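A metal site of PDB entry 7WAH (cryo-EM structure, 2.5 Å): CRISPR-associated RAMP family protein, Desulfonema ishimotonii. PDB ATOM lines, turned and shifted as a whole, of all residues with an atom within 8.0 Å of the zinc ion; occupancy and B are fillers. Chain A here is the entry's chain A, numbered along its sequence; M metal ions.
SG of Cys 86 sits close to N of Gly 88 (3.1 Å). The backbone carbonyl oxygen (O) of Cys 86 sits at hydrogen-bond distance from the indole nitrogen (NE1) of Trp 109, at 3.1 Å. SG of Cys 123 sits close to N of Phe 125 (3.5 Å). O of Cys 126 sits at hydrogen-bond distance from N of Arg 131. The guanidinium group (NH2) of Arg 131 lies within hydrogen-bond range of the backbone carbonyl oxygen (O) of Cys 115 (3.1 Å).
Four residues have an atom within 4 Å of the zinc ion: Cys 86, Cys 115, Cys 123 and Cys 126.
The zinc ion is bound by the side-chain sulfur of Cys 86 (2.3 Å), the side-chain sulfur of Cys 123 (2.3 Å), the side-chain sulfur of Cys 126 (2.3 Å) and the side-chain sulfur of Cys 115 (2.3 Å).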
ATOM      1  N   THR A  84     -18.329   2.398  28.832  1.00  0.00           N
ATOM      2  CA  THR A  84     -19.455   1.507  29.112  1.00  0.00           C
ATOM      3  C   THR A  84     -18.949   0.071  29.060  1.00  0.00           C
ATOM      4  O   THR A  84     -18.318  -0.338  28.067  1.00  0.00           O
ATOM      5  CB  THR A  84     -20.583   1.711  28.099  1.00  0.00           C
ATOM      6  OG1 THR A  84     -20.150   1.295  26.800  1.00  0.00           O
ATOM      7  CG2 THR A  84     -20.982   3.171  28.042  1.00  0.00           C
ATOM      8  N   CYS A  85     -19.221  -0.695  30.104  1.00  0.00           N
ATOM      9  CA  CYS A  85     -18.800  -2.089  30.157  1.00  0.00           C
ATOM     10  C   CYS A  85     -19.702  -2.955  29.290  1.00  0.00           C
ATOM     11  O   CYS A  85     -20.843  -2.612  28.986  1.00  0.00           O
ATOM     12  CB  CYS A  85     -18.809  -2.605  31.586  1.00  0.00           C
ATOM     13  SG  CYS A  85     -17.392  -2.092  32.582  1.00  0.00           S
ATOM     14  N   CYS A  86     -19.158  -4.108  28.881  1.00  0.00           N
ATOM     15  CA  CYS A  86     -19.905  -5.115  28.151  1.00  0.00           C
ATOM     16  C   CYS A  86     -20.720  -5.918  29.149  1.00  0.00           C
ATOM     17  O   CYS A  86     -20.520  -5.755  30.368  1.00  0.00           O
ATOM     18  CB  CYS A  86     -18.947  -6.009  27.351  1.00  0.00           C
ATOM     19  SG  CYS A  86     -18.276  -7.408  28.260  1.00  0.00           S
ATOM     20  N   PRO A  87     -21.658  -6.777  28.722  1.00  0.00           N
ATOM     21  CA  PRO A  87     -22.415  -7.577  29.690  1.00  0.00           C
ATOM     22  C   PRO A  87     -21.550  -8.528  30.508  1.00  0.00           C
ATOM     23  O   PRO A  87     -22.028  -9.074  31.509  1.00  0.00           O
ATOM     24  CB  PRO A  87     -23.408  -8.342  28.818  1.00  0.00           C
ATOM     25  CG  PRO A  87     -22.775  -8.384  27.490  1.00  0.00           C
ATOM     26  CD  PRO A  87     -22.109  -7.054  27.341  1.00  0.00           C
ATOM     27  N   GLY A  88     -20.304  -8.742  30.112  1.00  0.00           N
ATOM     28  CA  GLY A  88     -19.425  -9.645  30.820  1.00  0.00           C
ATOM     29  C   GLY A  88     -19.404 -11.016  30.185  1.00  0.00           C
ATOM     30  O   GLY A  88     -20.395 -11.495  29.621  1.00  0.00           O
ATOM     31  N   LYS A  89     -18.243 -11.663  30.266  1.00  0.00           N
ATOM     32  CA  LYS A  89     -18.052 -12.965  29.650  1.00  0.00           C
ATOM     33  C   LYS A  89     -17.810 -14.001  30.733  1.00  0.00           C
ATOM     34  O   LYS A  89     -16.758 -13.995  31.392  1.00  0.00           O
ATOM     35  CB  LYS A  89     -16.890 -12.941  28.658  1.00  0.00           C
ATOM     36  CG  LYS A  89     -16.590 -14.276  28.011  1.00  0.00           C
ATOM     37  CD  LYS A  89     -15.950 -14.105  26.652  1.00  0.00           C
ATOM     38  CE  LYS A  89     -15.430 -15.431  26.122  1.00  0.00           C
ATOM     39  NZ  LYS A  89     -16.476 -16.479  26.135  1.00  0.00           N
ATOM     40  N   TRP A 109     -26.997  -5.725  32.868  1.00  0.00           N
ATOM     41  CA  TRP A 109     -27.089  -4.283  32.808  1.00  0.00           C
ATOM     42  C   TRP A 109     -27.092  -3.728  31.389  1.00  0.00           C
ATOM     43  O   TRP A 109     -27.230  -2.516  31.216  1.00  0.00           O
ATOM     44  CB  TRP A 109     -25.943  -3.636  33.596  1.00  0.00           C
ATOM     45  CG  TRP A 109     -24.587  -4.131  33.211  1.00  0.00           C
ATOM     46  CD1 TRP A 109     -23.814  -3.688  32.174  1.00  0.00           C
ATOM     47  CD2 TRP A 109     -23.845  -5.179  33.848  1.00  0.00           C
ATOM     48  NE1 TRP A 109     -22.635  -4.388  32.132  1.00  0.00           N
ATOM     49  CE2 TRP A 109     -22.634  -5.314  33.147  1.00  0.00           C
ATOM     50  CE3 TRP A 109     -24.086  -6.022  34.937  1.00  0.00           C
ATOM     51  CZ2 TRP A 109     -21.655  -6.246  33.498  1.00  0.00           C
ATOM     52  CZ3 TRP A 109     -23.127  -6.945  35.287  1.00  0.00           C
ATOM     53  CH2 TRP A 109     -21.923  -7.054  34.572  1.00  0.00           C
ATOM     54  N   ASN A 113     -23.646  -7.353  22.969  1.00  0.00           N
ATOM     55  CA  ASN A 113     -22.898  -8.595  22.931  1.00  0.00           C
ATOM     56  C   ASN A 113     -21.628  -8.460  23.759  1.00  0.00           C
ATOM     57  O   ASN A 113     -21.055  -7.377  23.849  1.00  0.00           O
ATOM     58  CB  ASN A 113     -22.544  -8.956  21.482  1.00  0.00           C
ATOM     59  CG  ASN A 113     -21.987 -10.356  21.335  1.00  0.00           C
ATOM     60  OD1 ASN A 113     -22.729 -11.308  21.135  1.00  0.00           O
ATOM     61  ND2 ASN A 113     -20.668 -10.481  21.442  1.00  0.00           N
ATOM     62  N   PRO A 114     -21.173  -9.541  24.397  1.00  0.00           N
ATOM     63  CA  PRO A 114     -19.901  -9.478  25.125  1.00  0.00           C
ATOM     64  C   PRO A 114     -18.741  -9.167  24.191  1.00  0.00           C
ATOM     65  O   PRO A 114     -18.837  -9.289  22.966  1.00  0.00           O
ATOM     66  CB  PRO A 114     -19.768 -10.882  25.738  1.00  0.00           C
ATOM     67  CG  PRO A 114     -20.747 -11.741  24.988  1.00  0.00           C
ATOM     68  CD  PRO A 114     -21.864 -10.821  24.612  1.00  0.00           C
ATOM     69  N   CYS A 115     -17.636  -8.746  24.792  1.00  0.00           N
ATOM     70  CA  CYS A 115     -16.485  -8.304  24.033  1.00  0.00           C
ATOM     71  C   CYS A 115     -15.941  -9.439  23.164  1.00  0.00           C
ATOM     72  O   CYS A 115     -16.042 -10.621  23.534  1.00  0.00           O
ATOM     73  CB  CYS A 115     -15.381  -7.782  24.962  1.00  0.00           C
ATOM     74  SG  CYS A 115     -15.745  -6.180  25.712  1.00  0.00           S
ATOM     75  N   PRO A 116     -15.366  -9.129  22.003  1.00  0.00           N
ATOM     76  CA  PRO A 116     -14.832 -10.179  21.130  1.00  0.00           C
ATOM     77  C   PRO A 116     -13.709 -10.944  21.800  1.00  0.00           C
ATOM     78  O   PRO A 116     -12.989 -10.416  22.657  1.00  0.00           O
ATOM     79  CB  PRO A 116     -14.325  -9.396  19.905  1.00  0.00           C
ATOM     80  CG  PRO A 116     -15.073  -8.110  19.937  1.00  0.00           C
ATOM     81  CD  PRO A 116     -15.264  -7.793  21.395  1.00  0.00           C
ATOM     82  N   THR A 121      -8.605  -3.711  22.144  1.00  0.00           N
ATOM     83  CA  THR A 121      -8.871  -3.187  23.475  1.00  0.00           C
ATOM     84  C   THR A 121     -10.052  -3.921  24.091  1.00  0.00           C
ATOM     85  O   THR A 121     -10.949  -4.407  23.383  1.00  0.00           O
ATOM     86  CB  THR A 121      -9.156  -1.677  23.451  1.00  0.00           C
ATOM     87  OG1 THR A 121      -9.450  -1.226  24.772  1.00  0.00           O
ATOM     88  CG2 THR A 121     -10.325  -1.361  22.535  1.00  0.00           C
ATOM     89  N   TYR A 122     -10.049  -4.010  25.416  1.00  0.00           N
ATOM     90  CA  TYR A 122     -11.107  -4.666  26.173  1.00  0.00           C
ATOM     91  C   TYR A 122     -11.751  -3.662  27.125  1.00  0.00           C
ATOM     92  O   TYR A 122     -11.097  -2.719  27.584  1.00  0.00           O
ATOM     93  CB  TYR A 122     -10.585  -5.868  26.967  1.00  0.00           C
ATOM     94  CG  TYR A 122     -10.064  -6.997  26.106  1.00  0.00           C
ATOM     95  CD1 TYR A 122      -8.740  -7.005  25.681  1.00  0.00           C
ATOM     96  CD2 TYR A 122     -10.891  -8.047  25.733  1.00  0.00           C
ATOM     97  CE1 TYR A 122      -8.257  -8.037  24.900  1.00  0.00           C
ATOM     98  CE2 TYR A 122     -10.418  -9.079  24.950  1.00  0.00           C
ATOM     99  CZ  TYR A 122      -9.095  -9.068  24.532  1.00  0.00           C
ATOM    100  OH  TYR A 122      -8.622 -10.100  23.749  1.00  0.00           O
ATOM    101  N   CYS A 123     -13.028  -3.886  27.434  1.00  0.00           N
ATOM    102  CA  CYS A 123     -13.717  -3.072  28.406  1.00  0.00           C
ATOM    103  C   CYS A 123     -13.113  -3.295  29.795  1.00  0.00           C
ATOM    104  O   CYS A 123     -12.457  -4.320  30.031  1.00  0.00           O
ATOM    105  CB  CYS A 123     -15.204  -3.402  28.415  1.00  0.00           C
ATOM    106  SG  CYS A 123     -15.633  -4.910  29.301  1.00  0.00           S
ATOM    107  N   PRO A 124     -13.310  -2.352  30.716  1.00  0.00           N
ATOM    108  CA  PRO A 124     -12.749  -2.533  32.066  1.00  0.00           C
ATOM    109  C   PRO A 124     -13.225  -3.805  32.744  1.00  0.00           C
ATOM    110  O   PRO A 124     -12.462  -4.409  33.511  1.00  0.00           O
ATOM    111  CB  PRO A 124     -13.224  -1.276  32.809  1.00  0.00           C
ATOM    112  CG  PRO A 124     -13.417  -0.271  31.736  1.00  0.00           C
ATOM    113  CD  PRO A 124     -13.910  -1.018  30.548  1.00  0.00           C
ATOM    114  N   PHE A 125     -14.462  -4.222  32.505  1.00  0.00           N
ATOM    115  CA  PHE A 125     -14.967  -5.447  33.129  1.00  0.00           C
ATOM    116  C   PHE A 125     -14.200  -6.671  32.636  1.00  0.00           C
ATOM    117  O   PHE A 125     -13.861  -7.558  33.425  1.00  0.00           O
ATOM    118  CB  PHE A 125     -16.463  -5.595  32.853  1.00  0.00           C
ATOM    119  CG  PHE A 125     -17.144  -6.580  33.761  1.00  0.00           C
ATOM    120  CD1 PHE A 125     -16.914  -6.558  35.121  1.00  0.00           C
ATOM    121  CD2 PHE A 125     -18.034  -7.514  33.253  1.00  0.00           C
ATOM    122  CE1 PHE A 125     -17.540  -7.462  35.962  1.00  0.00           C
ATOM    123  CE2 PHE A 125     -18.667  -8.416  34.082  1.00  0.00           C
ATOM    124  CZ  PHE A 125     -18.425  -8.390  35.435  1.00  0.00           C
ATOM    125  N   CYS A 126     -13.910  -6.736  31.332  1.00  0.00           N
ATOM    126  CA  CYS A 126     -13.135  -7.852  30.803  1.00  0.00           C
ATOM    127  C   CYS A 126     -11.702  -7.842  31.319  1.00  0.00           C
ATOM    128  O   CYS A 126     -11.121  -8.899  31.570  1.00  0.00           O
ATOM    129  CB  CYS A 126     -13.154  -7.834  29.276  1.00  0.00           C
ATOM    130  SG  CYS A 126     -14.659  -8.505  28.541  1.00  0.00           S
ATOM    131  N   GLU A 127     -11.116  -6.655  31.481  1.00  0.00           N
ATOM    132  CA  GLU A 127      -9.792  -6.562  32.068  1.00  0.00           C
ATOM    133  C   GLU A 127      -9.794  -7.050  33.509  1.00  0.00           C
ATOM    134  O   GLU A 127      -8.864  -7.750  33.943  1.00  0.00           O
ATOM    135  CB  GLU A 127      -9.277  -5.123  32.000  1.00  0.00           C
ATOM    136  CG  GLU A 127      -9.287  -4.515  30.610  1.00  0.00           C
ATOM    137  CD  GLU A 127      -8.708  -3.114  30.575  1.00  0.00           C
ATOM    138  OE1 GLU A 127      -7.637  -2.901  31.192  1.00  0.00           O
ATOM    139  OE2 GLU A 127      -9.319  -2.230  29.952  1.00  0.00           O
ATOM    140  N   LEU A 129     -11.898  -9.250  34.743  1.00  0.00           N
ATOM    141  CA  LEU A 129     -12.063 -10.699  34.668  1.00  0.00           C
ATOM    142  C   LEU A 129     -10.731 -11.378  34.353  1.00  0.00           C
ATOM    143  O   LEU A 129     -10.462 -12.480  34.855  1.00  0.00           O
ATOM    144  CB  LEU A 129     -13.108 -11.058  33.615  1.00  0.00           C
ATOM    145  CG  LEU A 129     -14.549 -10.656  33.915  1.00  0.00           C
ATOM    146  CD1 LEU A 129     -15.457 -11.042  32.753  1.00  0.00           C
ATOM    147  CD2 LEU A 129     -15.027 -11.297  35.197  1.00  0.00           C
ATOM    148  N   ARG A 131      -9.450 -11.340  30.844  1.00  0.00           N
ATOM    149  CA  ARG A 131      -9.361 -11.670  29.434  1.00  0.00           C
ATOM    150  C   ARG A 131      -8.284 -10.851  28.729  1.00  0.00           C
ATOM    151  O   ARG A 131      -7.634 -11.352  27.794  1.00  0.00           O
ATOM    152  CB  ARG A 131     -10.704 -11.456  28.747  1.00  0.00           C
ATOM    153  CG  ARG A 131     -11.821 -12.353  29.264  1.00  0.00           C
ATOM    154  CD  ARG A 131     -13.114 -12.046  28.534  1.00  0.00           C
ATOM    155  NE  ARG A 131     -12.916 -12.050  27.091  1.00  0.00           N
ATOM    156  CZ  ARG A 131     -13.767 -11.544  26.215  1.00  0.00           C
ATOM    157  NH1 ARG A 131     -14.900 -10.969  26.602  1.00  0.00           N
ATOM    158  NH2 ARG A 131     -13.489 -11.622  24.915  1.00  0.00           N
HETATM  159 ZN    ZN M   1     -16.068  -6.752  27.953  1.00  0.00          ZN
